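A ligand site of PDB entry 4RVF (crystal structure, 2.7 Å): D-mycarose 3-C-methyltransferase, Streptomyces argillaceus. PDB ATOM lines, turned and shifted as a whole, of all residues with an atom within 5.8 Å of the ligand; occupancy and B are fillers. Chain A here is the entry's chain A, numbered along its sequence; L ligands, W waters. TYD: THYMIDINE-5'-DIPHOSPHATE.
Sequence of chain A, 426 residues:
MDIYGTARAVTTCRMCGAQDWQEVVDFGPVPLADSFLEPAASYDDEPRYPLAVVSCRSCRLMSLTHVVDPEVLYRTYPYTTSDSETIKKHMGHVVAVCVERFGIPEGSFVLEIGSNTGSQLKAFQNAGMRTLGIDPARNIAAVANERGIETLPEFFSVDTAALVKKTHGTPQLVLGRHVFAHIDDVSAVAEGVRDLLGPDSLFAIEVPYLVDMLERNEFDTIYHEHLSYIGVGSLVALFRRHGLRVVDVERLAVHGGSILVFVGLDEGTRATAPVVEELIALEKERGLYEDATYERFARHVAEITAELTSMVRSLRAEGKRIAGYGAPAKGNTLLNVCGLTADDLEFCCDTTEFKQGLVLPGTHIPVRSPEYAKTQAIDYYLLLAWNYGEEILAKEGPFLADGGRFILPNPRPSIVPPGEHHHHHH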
ATOM      1  N   ASP A  34      36.573 -22.096 -22.079  1.00  0.00           N
ATOM      2  CA  ASP A  34      36.246 -22.993 -20.961  1.00  0.00           C
ATOM      3  C   ASP A  34      36.472 -22.370 -19.575  1.00  0.00           C
ATOM      4  O   ASP A  34      36.463 -23.069 -18.563  1.00  0.00           O
ATOM      5  CB  ASP A  34      37.045 -24.308 -21.078  1.00  0.00           C
ATOM      6  CG  ASP A  34      36.325 -25.364 -21.918  1.00  0.00           C
ATOM      7  OD1 ASP A  34      35.284 -25.051 -22.547  1.00  0.00           O
ATOM      8  OD2 ASP A  34      36.812 -26.519 -21.958  1.00  0.00           O
ATOM      9  N   SER A  84      26.781 -38.449 -23.617  1.00  0.00           N
ATOM     10  CA  SER A  84      25.723 -38.564 -24.609  1.00  0.00           C
ATOM     11  C   SER A  84      25.611 -39.986 -25.110  1.00  0.00           C
ATOM     12  O   SER A  84      26.579 -40.760 -25.072  1.00  0.00           O
ATOM     13  CB  SER A  84      26.024 -37.645 -25.806  1.00  0.00           C
ATOM     14  OG  SER A  84      27.016 -36.673 -25.503  1.00  0.00           O
ATOM     15  N   ILE A  87      28.008 -40.063 -27.909  1.00  0.00           N
ATOM     16  CA  ILE A  87      29.411 -40.344 -27.634  1.00  0.00           C
ATOM     17  C   ILE A  87      29.656 -41.815 -27.380  1.00  0.00           C
ATOM     18  O   ILE A  87      30.642 -42.370 -27.848  1.00  0.00           O
ATOM     19  CB  ILE A  87      29.899 -39.561 -26.394  1.00  0.00           C
ATOM     20  CG1 ILE A  87      29.819 -38.055 -26.668  1.00  0.00           C
ATOM     21  CG2 ILE A  87      31.343 -39.918 -26.049  1.00  0.00           C
ATOM     22  CD1 ILE A  87      30.444 -37.634 -27.987  1.00  0.00           C
ATOM     23  N   HIS A 178      41.478 -35.318 -30.365  1.00  0.00           N
ATOM     24  CA  HIS A 178      41.565 -33.905 -29.934  1.00  0.00           C
ATOM     25  C   HIS A 178      42.973 -33.545 -29.494  1.00  0.00           C
ATOM     26  O   HIS A 178      43.557 -32.592 -30.013  1.00  0.00           O
ATOM     27  CB  HIS A 178      40.569 -33.604 -28.801  1.00  0.00           C
ATOM     28  CG  HIS A 178      39.156 -33.921 -29.162  1.00  0.00           C
ATOM     29  ND1 HIS A 178      38.358 -34.734 -28.394  1.00  0.00           N
ATOM     30  CD2 HIS A 178      38.416 -33.546 -30.231  1.00  0.00           C
ATOM     31  CE1 HIS A 178      37.173 -34.836 -28.968  1.00  0.00           C
ATOM     32  NE2 HIS A 178      37.178 -34.126 -30.086  1.00  0.00           N
ATOM     33  N   TYR A 223      38.680 -21.717 -31.119  1.00  0.00           N
ATOM     34  CA  TYR A 223      38.960 -21.195 -29.791  1.00  0.00           C
ATOM     35  C   TYR A 223      40.331 -21.653 -29.335  1.00  0.00           C
ATOM     36  O   TYR A 223      40.936 -22.560 -29.927  1.00  0.00           O
ATOM     37  CB  TYR A 223      37.864 -21.554 -28.783  1.00  0.00           C
ATOM     38  CG  TYR A 223      37.375 -22.984 -28.802  1.00  0.00           C
ATOM     39  CD1 TYR A 223      37.886 -23.914 -27.895  1.00  0.00           C
ATOM     40  CD2 TYR A 223      36.386 -23.398 -29.689  1.00  0.00           C
ATOM     41  CE1 TYR A 223      37.440 -25.232 -27.890  1.00  0.00           C
ATOM     42  CE2 TYR A 223      35.937 -24.708 -29.690  1.00  0.00           C
ATOM     43  CZ  TYR A 223      36.460 -25.612 -28.787  1.00  0.00           C
ATOM     44  OH  TYR A 223      36.011 -26.916 -28.780  1.00  0.00           O
ATOM     45  N   HIS A 255      31.500 -33.958 -34.257  1.00  0.00           N
ATOM     46  CA  HIS A 255      32.164 -32.663 -34.052  1.00  0.00           C
ATOM     47  C   HIS A 255      32.111 -31.772 -35.302  1.00  0.00           C
ATOM     48  O   HIS A 255      33.062 -31.062 -35.616  1.00  0.00           O
ATOM     49  CB  HIS A 255      33.598 -32.864 -33.561  1.00  0.00           C
ATOM     50  CG  HIS A 255      33.675 -33.608 -32.265  1.00  0.00           C
ATOM     51  ND1 HIS A 255      33.320 -33.038 -31.059  1.00  0.00           N
ATOM     52  CD2 HIS A 255      34.062 -34.874 -31.980  1.00  0.00           C
ATOM     53  CE1 HIS A 255      33.476 -33.920 -30.098  1.00  0.00           C
ATOM     54  NE2 HIS A 255      33.932 -35.044 -30.627  1.00  0.00           N
ATOM     55  N   TYR A 325      20.786 -23.054 -26.026  1.00  0.00           N
ATOM     56  CA  TYR A 325      20.679 -24.485 -25.713  1.00  0.00           C
ATOM     57  C   TYR A 325      22.075 -25.073 -25.677  1.00  0.00           C
ATOM     58  O   TYR A 325      22.755 -25.155 -26.701  1.00  0.00           O
ATOM     59  CB  TYR A 325      19.818 -25.208 -26.751  1.00  0.00           C
ATOM     60  CG  TYR A 325      19.269 -26.548 -26.300  1.00  0.00           C
ATOM     61  CD1 TYR A 325      20.101 -27.657 -26.117  1.00  0.00           C
ATOM     62  CD2 TYR A 325      17.910 -26.719 -26.048  1.00  0.00           C
ATOM     63  CE1 TYR A 325      19.597 -28.880 -25.707  1.00  0.00           C
ATOM     64  CE2 TYR A 325      17.404 -27.941 -25.652  1.00  0.00           C
ATOM     65  CZ  TYR A 325      18.248 -29.017 -25.466  1.00  0.00           C
ATOM     66  OH  TYR A 325      17.747 -30.222 -25.068  1.00  0.00           O
ATOM     67  N   GLY A 326      22.505 -25.490 -24.487  1.00  0.00           N
ATOM     68  CA  GLY A 326      23.885 -25.924 -24.267  1.00  0.00           C
ATOM     69  C   GLY A 326      24.826 -24.743 -24.041  1.00  0.00           C
ATOM     70  O   GLY A 326      24.563 -23.634 -24.498  1.00  0.00           O
ATOM     71  N   ALA A 327      25.914 -25.006 -23.333  1.00  0.00           N
ATOM     72  CA  ALA A 327      26.965 -24.013 -23.101  1.00  0.00           C
ATOM     73  C   ALA A 327      28.350 -24.594 -23.437  1.00  0.00           C
ATOM     74  O   ALA A 327      29.223 -24.647 -22.580  1.00  0.00           O
ATOM     75  CB  ALA A 327      26.916 -23.543 -21.660  1.00  0.00           C
ATOM     76  N   PRO A 328      28.541 -25.020 -24.699  1.00  0.00           N
ATOM     77  CA  PRO A 328      29.826 -25.572 -25.103  1.00  0.00           C
ATOM     78  C   PRO A 328      30.855 -24.469 -25.364  1.00  0.00           C
ATOM     79  O   PRO A 328      30.503 -23.294 -25.472  1.00  0.00           O
ATOM     80  CB  PRO A 328      29.495 -26.300 -26.402  1.00  0.00           C
ATOM     81  CG  PRO A 328      28.374 -25.526 -26.980  1.00  0.00           C
ATOM     82  CD  PRO A 328      27.585 -24.994 -25.815  1.00  0.00           C
ATOM     83  N   ALA A 329      32.119 -24.880 -25.477  1.00  0.00           N
ATOM     84  CA  ALA A 329      33.216 -23.948 -25.759  1.00  0.00           C
ATOM     85  C   ALA A 329      32.921 -23.078 -26.982  1.00  0.00           C
ATOM     86  O   ALA A 329      33.057 -21.863 -26.934  1.00  0.00           O
ATOM     87  CB  ALA A 329      34.505 -24.718 -25.950  1.00  0.00           C
ATOM     88  N   LYS A 330      32.513 -23.724 -28.077  1.00  0.00           N
ATOM     89  CA  LYS A 330      32.233 -23.023 -29.327  1.00  0.00           C
ATOM     90  C   LYS A 330      31.149 -21.944 -29.209  1.00  0.00           C
ATOM     91  O   LYS A 330      31.174 -20.951 -29.935  1.00  0.00           O
ATOM     92  CB  LYS A 330      31.861 -24.006 -30.440  1.00  0.00           C
ATOM     93  CG  LYS A 330      30.568 -24.763 -30.226  1.00  0.00           C
ATOM     94  CD  LYS A 330      30.239 -25.611 -31.442  1.00  0.00           C
ATOM     95  CE  LYS A 330      29.876 -27.036 -31.060  1.00  0.00           C
ATOM     96  NZ  LYS A 330      31.059 -27.811 -30.585  1.00  0.00           N
ATOM     97  N   CSO A 349      20.760 -22.919 -21.097  1.00  0.00           N
ATOM     98  CA  CSO A 349      20.510 -24.177 -20.369  1.00  0.00           C
ATOM     99  CB  CSO A 349      19.130 -24.767 -20.695  1.00  0.00           C
ATOM    100  SG  CSO A 349      18.995 -25.457 -22.307  1.00  0.00           S
ATOM    101  C   CSO A 349      21.652 -25.120 -20.649  1.00  0.00           C
ATOM    102  O   CSO A 349      22.197 -25.127 -21.751  1.00  0.00           O
ATOM    103  OD  CSO A 349      18.917 -27.172 -22.025  1.00  0.00           O
ATOM    104  N   ASP A 350      22.046 -25.907 -19.646  1.00  0.00           N
ATOM    105  CA  ASP A 350      23.133 -26.870 -19.820  1.00  0.00           C
ATOM    106  C   ASP A 350      23.049 -28.033 -18.835  1.00  0.00           C
ATOM    107  O   ASP A 350      22.794 -27.841 -17.649  1.00  0.00           O
ATOM    108  CB  ASP A 350      24.484 -26.162 -19.725  1.00  0.00           C
ATOM    109  CG  ASP A 350      25.642 -27.062 -20.131  1.00  0.00           C
ATOM    110  OD1 ASP A 350      26.062 -27.897 -19.312  1.00  0.00           O
ATOM    111  OD2 ASP A 350      26.139 -26.920 -21.269  1.00  0.00           O
ATOM    112  N   THR A 351      23.302 -29.240 -19.338  1.00  0.00           N
ATOM    113  CA  THR A 351      23.197 -30.464 -18.533  1.00  0.00           C
ATOM    114  C   THR A 351      24.363 -30.650 -17.565  1.00  0.00           C
ATOM    115  O   THR A 351      24.198 -31.313 -16.545  1.00  0.00           O
ATOM    116  CB  THR A 351      23.119 -31.721 -19.426  1.00  0.00           C
ATOM    117  OG1 THR A 351      24.258 -31.771 -20.292  1.00  0.00           O
ATOM    118  CG2 THR A 351      21.835 -31.721 -20.252  1.00  0.00           C
ATOM    119  N   THR A 352      25.520 -30.069 -17.878  1.00  0.00           N
ATOM    120  CA  THR A 352      26.700 -30.201 -17.020  1.00  0.00           C
ATOM    121  C   THR A 352      26.475 -29.465 -15.709  1.00  0.00           C
ATOM    122  O   THR A 352      26.144 -28.278 -15.688  1.00  0.00           O
ATOM    123  CB  THR A 352      27.972 -29.681 -17.707  1.00  0.00           C
ATOM    124  OG1 THR A 352      28.126 -30.308 -18.991  1.00  0.00           O
ATOM    125  CG2 THR A 352      29.211 -29.981 -16.860  1.00  0.00           C
ATOM    126  N   LYS A 355      28.744 -26.393 -14.576  1.00  0.00           N
ATOM    127  CA  LYS A 355      28.422 -25.132 -15.255  1.00  0.00           C
ATOM    128  C   LYS A 355      27.152 -24.449 -14.733  1.00  0.00           C
ATOM    129  O   LYS A 355      27.053 -23.220 -14.791  1.00  0.00           O
ATOM    130  CB  LYS A 355      28.286 -25.363 -16.770  1.00  0.00           C
ATOM    131  CG  LYS A 355      29.563 -25.843 -17.445  1.00  0.00           C
ATOM    132  CD  LYS A 355      29.355 -26.063 -18.926  1.00  0.00           C
ATOM    133  CE  LYS A 355      30.564 -26.726 -19.566  1.00  0.00           C
ATOM    134  NZ  LYS A 355      30.410 -26.849 -21.049  1.00  0.00           N
ATOM    135  N   ALA A 385      25.034 -25.980 -29.065  1.00  0.00           N
ATOM    136  CA  ALA A 385      25.536 -27.355 -29.182  1.00  0.00           C
ATOM    137  C   ALA A 385      25.001 -28.026 -30.456  1.00  0.00           C
ATOM    138  O   ALA A 385      24.487 -29.137 -30.418  1.00  0.00           O
ATOM    139  CB  ALA A 385      25.132 -28.166 -27.960  1.00  0.00           C
ATOM    140  N   ASN A 387      26.350 -29.446 -32.976  1.00  0.00           N
ATOM    141  CA  ASN A 387      26.930 -30.730 -33.380  1.00  0.00           C
ATOM    142  C   ASN A 387      26.200 -31.934 -32.774  1.00  0.00           C
ATOM    143  O   ASN A 387      26.322 -33.047 -33.258  1.00  0.00           O
ATOM    144  CB  ASN A 387      28.448 -30.794 -33.098  1.00  0.00           C
ATOM    145  CG  ASN A 387      28.790 -30.676 -31.629  1.00  0.00           C
ATOM    146  OD1 ASN A 387      28.431 -29.691 -30.969  1.00  0.00           O
ATOM    147  ND2 ASN A 387      29.508 -31.665 -31.101  1.00  0.00           N
ATOM    148  N   TYR A 388      25.411 -31.687 -31.716  1.00  0.00           N
ATOM    149  CA  TYR A 388      24.502 -32.694 -31.155  1.00  0.00           C
ATOM    150  C   TYR A 388      23.038 -32.471 -31.567  1.00  0.00           C
ATOM    151  O   TYR A 388      22.125 -32.891 -30.877  1.00  0.00           O
ATOM    152  CB  TYR A 388      24.598 -32.683 -29.637  1.00  0.00           C
ATOM    153  CG  TYR A 388      25.962 -33.059 -29.116  1.00  0.00           C
ATOM    154  CD1 TYR A 388      26.388 -34.382 -29.106  1.00  0.00           C
ATOM    155  CD2 TYR A 388      26.836 -32.087 -28.629  1.00  0.00           C
ATOM    156  CE1 TYR A 388      27.634 -34.735 -28.637  1.00  0.00           C
ATOM    157  CE2 TYR A 388      28.088 -32.424 -28.159  1.00  0.00           C
ATOM    158  CZ  TYR A 388      28.493 -33.751 -28.161  1.00  0.00           C
ATOM    159  OH  TYR A 388      29.740 -34.104 -27.692  1.00  0.00           O
ATOM    160  N   GLU A 391      20.425 -35.633 -31.656  1.00  0.00           N
ATOM    161  CA  GLU A 391      20.066 -36.096 -30.319  1.00  0.00           C
ATOM    162  C   GLU A 391      19.107 -35.122 -29.613  1.00  0.00           C
ATOM    163  O   GLU A 391      18.147 -35.540 -28.966  1.00  0.00           O
ATOM    164  CB  GLU A 391      21.337 -36.258 -29.479  1.00  0.00           C
ATOM    165  CG  GLU A 391      21.138 -36.980 -28.153  1.00  0.00           C
ATOM    166  CD  GLU A 391      22.405 -37.019 -27.301  1.00  0.00           C
ATOM    167  OE1 GLU A 391      22.322 -37.483 -26.143  1.00  0.00           O
ATOM    168  OE2 GLU A 391      23.468 -36.567 -27.779  1.00  0.00           O
ATOM    169  N   ILE A 392      19.389 -33.827 -29.742  1.00  0.00           N
ATOM    170  CA  ILE A 392      18.607 -32.789 -29.075  1.00  0.00           C
ATOM    171  C   ILE A 392      17.189 -32.678 -29.662  1.00  0.00           C
ATOM    172  O   ILE A 392      16.206 -32.634 -28.922  1.00  0.00           O
ATOM    173  CB  ILE A 392      19.327 -31.428 -29.144  1.00  0.00           C
ATOM    174  CG1 ILE A 392      20.577 -31.465 -28.247  1.00  0.00           C
ATOM    175  CG2 ILE A 392      18.419 -30.296 -28.691  1.00  0.00           C
ATOM    176  CD1 ILE A 392      21.598 -30.392 -28.562  1.00  0.00           C
ATOM    177  N   LYS A 395      14.579 -35.434 -28.688  1.00  0.00           N
ATOM    178  CA  LYS A 395      13.952 -35.387 -27.366  1.00  0.00           C
ATOM    179  C   LYS A 395      13.160 -34.098 -27.059  1.00  0.00           C
ATOM    180  O   LYS A 395      12.485 -34.036 -26.045  1.00  0.00           O
ATOM    181  CB  LYS A 395      14.995 -35.645 -26.275  1.00  0.00           C
ATOM    182  CG  LYS A 395      16.026 -34.539 -26.110  1.00  0.00           C
ATOM    183  CD  LYS A 395      17.111 -34.902 -25.112  1.00  0.00           C
ATOM    184  CE  LYS A 395      18.061 -33.722 -24.910  1.00  0.00           C
ATOM    185  NZ  LYS A 395      19.319 -34.106 -24.223  1.00  0.00           N
HETATM  186  PA  TYD L   1      31.473 -29.577 -25.169  1.00  0.00           P
HETATM  187  O1A TYD L   1      31.724 -30.831 -24.356  1.00  0.00           O
HETATM  188  O2A TYD L   1      31.910 -28.217 -24.653  1.00  0.00           O
HETATM  189  O3A TYD L   1      32.226 -29.759 -26.580  1.00  0.00           O
HETATM  190  PB  TYD L   1      31.671 -30.795 -27.688  1.00  0.00           P
HETATM  191  O1B TYD L   1      31.294 -32.025 -26.893  1.00  0.00           O
HETATM  192  O2B TYD L   1      30.511 -30.041 -28.292  1.00  0.00           O
HETATM  193  O3B TYD L   1      32.853 -30.978 -28.615  1.00  0.00           O
HETATM  194  O5' TYD L   1      29.910 -29.520 -25.597  1.00  0.00           O
HETATM  195  C5' TYD L   1      28.871 -30.216 -24.899  1.00  0.00           C
HETATM  196  C4' TYD L   1      28.038 -29.237 -24.075  1.00  0.00           C
HETATM  197  O4' TYD L   1      26.672 -29.243 -24.513  1.00  0.00           O
HETATM  198  C3' TYD L   1      28.006 -29.578 -22.581  1.00  0.00           C
HETATM  199  O3' TYD L   1      28.298 -28.407 -21.789  1.00  0.00           O
HETATM  200  C2' TYD L   1      26.591 -30.040 -22.291  1.00  0.00           C
HETATM  201  C1' TYD L   1      25.768 -29.445 -23.424  1.00  0.00           C
HETATM  202  N1  TYD L   1      24.614 -30.284 -23.798  1.00  0.00           N
HETATM  203  C2  TYD L   1      23.341 -30.055 -23.205  1.00  0.00           C
HETATM  204  O2  TYD L   1      23.191 -29.144 -22.363  1.00  0.00           O
HETATM  205  N3  TYD L   1      22.265 -30.786 -23.525  1.00  0.00           N
HETATM  206  C4  TYD L   1      22.351 -31.781 -24.413  1.00  0.00           C
HETATM  207  O4  TYD L   1      21.335 -32.456 -24.705  1.00  0.00           O
HETATM  208  C5  TYD L   1      23.665 -32.057 -25.056  1.00  0.00           C
HETATM  209  C5M TYD L   1      23.824 -33.166 -26.065  1.00  0.00           C
HETATM  210  C6  TYD L   1      24.749 -31.271 -24.699  1.00  0.00           C
HETATM  211  O   HOH W   1      32.469 -26.815 -28.362  1.00  0.00           O
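N of Thr 351 sits at hydrogen-bond distance from O2 of the ligand (3.0 Å).
An oxygen (O2A) of the ligand sits at hydrogen-bond distance from the backbone NH (N) of Ala 329.
The side-chain amino group (NZ) of Lys 355 sits at hydrogen-bond distance from an oxygen (O3') of the ligand (2.7 Å).
The side-chain hydroxyl (OH) of Tyr 388 sits at hydrogen-bond distance from an oxygen (O1B) of the ligand, 2.7 Å away.
ND1 of His 255 sits at hydrogen-bond distance from O3B of the ligand (3.2 Å).
An oxygen (O3') of the ligand lies within hydrogen-bond range of the side-chain carboxylate of Asp 350, 2.7 Å away.
An oxygen (O3') of the ligand is in hydrogen-bond range of the side-chain hydroxyl of Thr 352, 3.4 Å away.
NZ of Lys 330 is in salt-bridge range of O2B of the ligand (3.2 Å).
The side-chain amino group (NZ) of Lys 395 is in hydrogen-bond range of an oxygen (O4) of the ligand (2.6 Å).
ND2 of Asn 387 is in hydrogen-bond range of O2B of the ligand (3.4 Å).
The backbone carbonyl oxygen of Tyr 325 sits at hydrogen-bond distance from the backbone NH of Ala 385, 3.4 Å away.
N of Ala 327 lies within hydrogen-bond range of OD2 of Asp 350 (2.8 Å).
OD1 of Asn 387 lies close to NZ of Lys 330, at 3.3 Å.
NE2 of His 255 lies within hydrogen-bond range of NE2 of His 178 (3.4 Å).
The side-chain amino group (NZ) of Lys 355 sits at hydrogen-bond distance from the backbone carbonyl oxygen (O) of Ala 327 (2.9 Å).
O of CSO 349 is in hydrogen-bond range of N of Gly 326 (2.8 Å).
OD1 of Asp 350 lies within hydrogen-bond range of N of Thr 352, 2.7 Å away.
Merely in contact with the ligand: Tyr 325 (3.9 Å), Gly 326 (3.8 Å), Ala 327 (3.95 Å), Pro 328 (3.3 Å), Ala 385 (3.9 Å), Glu 391 (3.8 Å) and Ile 392 (3.8 Å).
Hydrophobic or aromatic side chains that line the ligand: His 255, Tyr 325, Pro 328, Ala 385, Tyr 388 and Ile 392.
Of the 23 residues printed, 17 come within 4 Å of the ligand.
The nearest printed residue that does not touch the ligand is CSO 349 (4.2 Å).
Water W1 lies within hydrogen-bond range of the side-chain amino group (NZ) of Lys 330, an oxygen (O3A) of the ligand and the backbone NH (N) of Ala 329.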
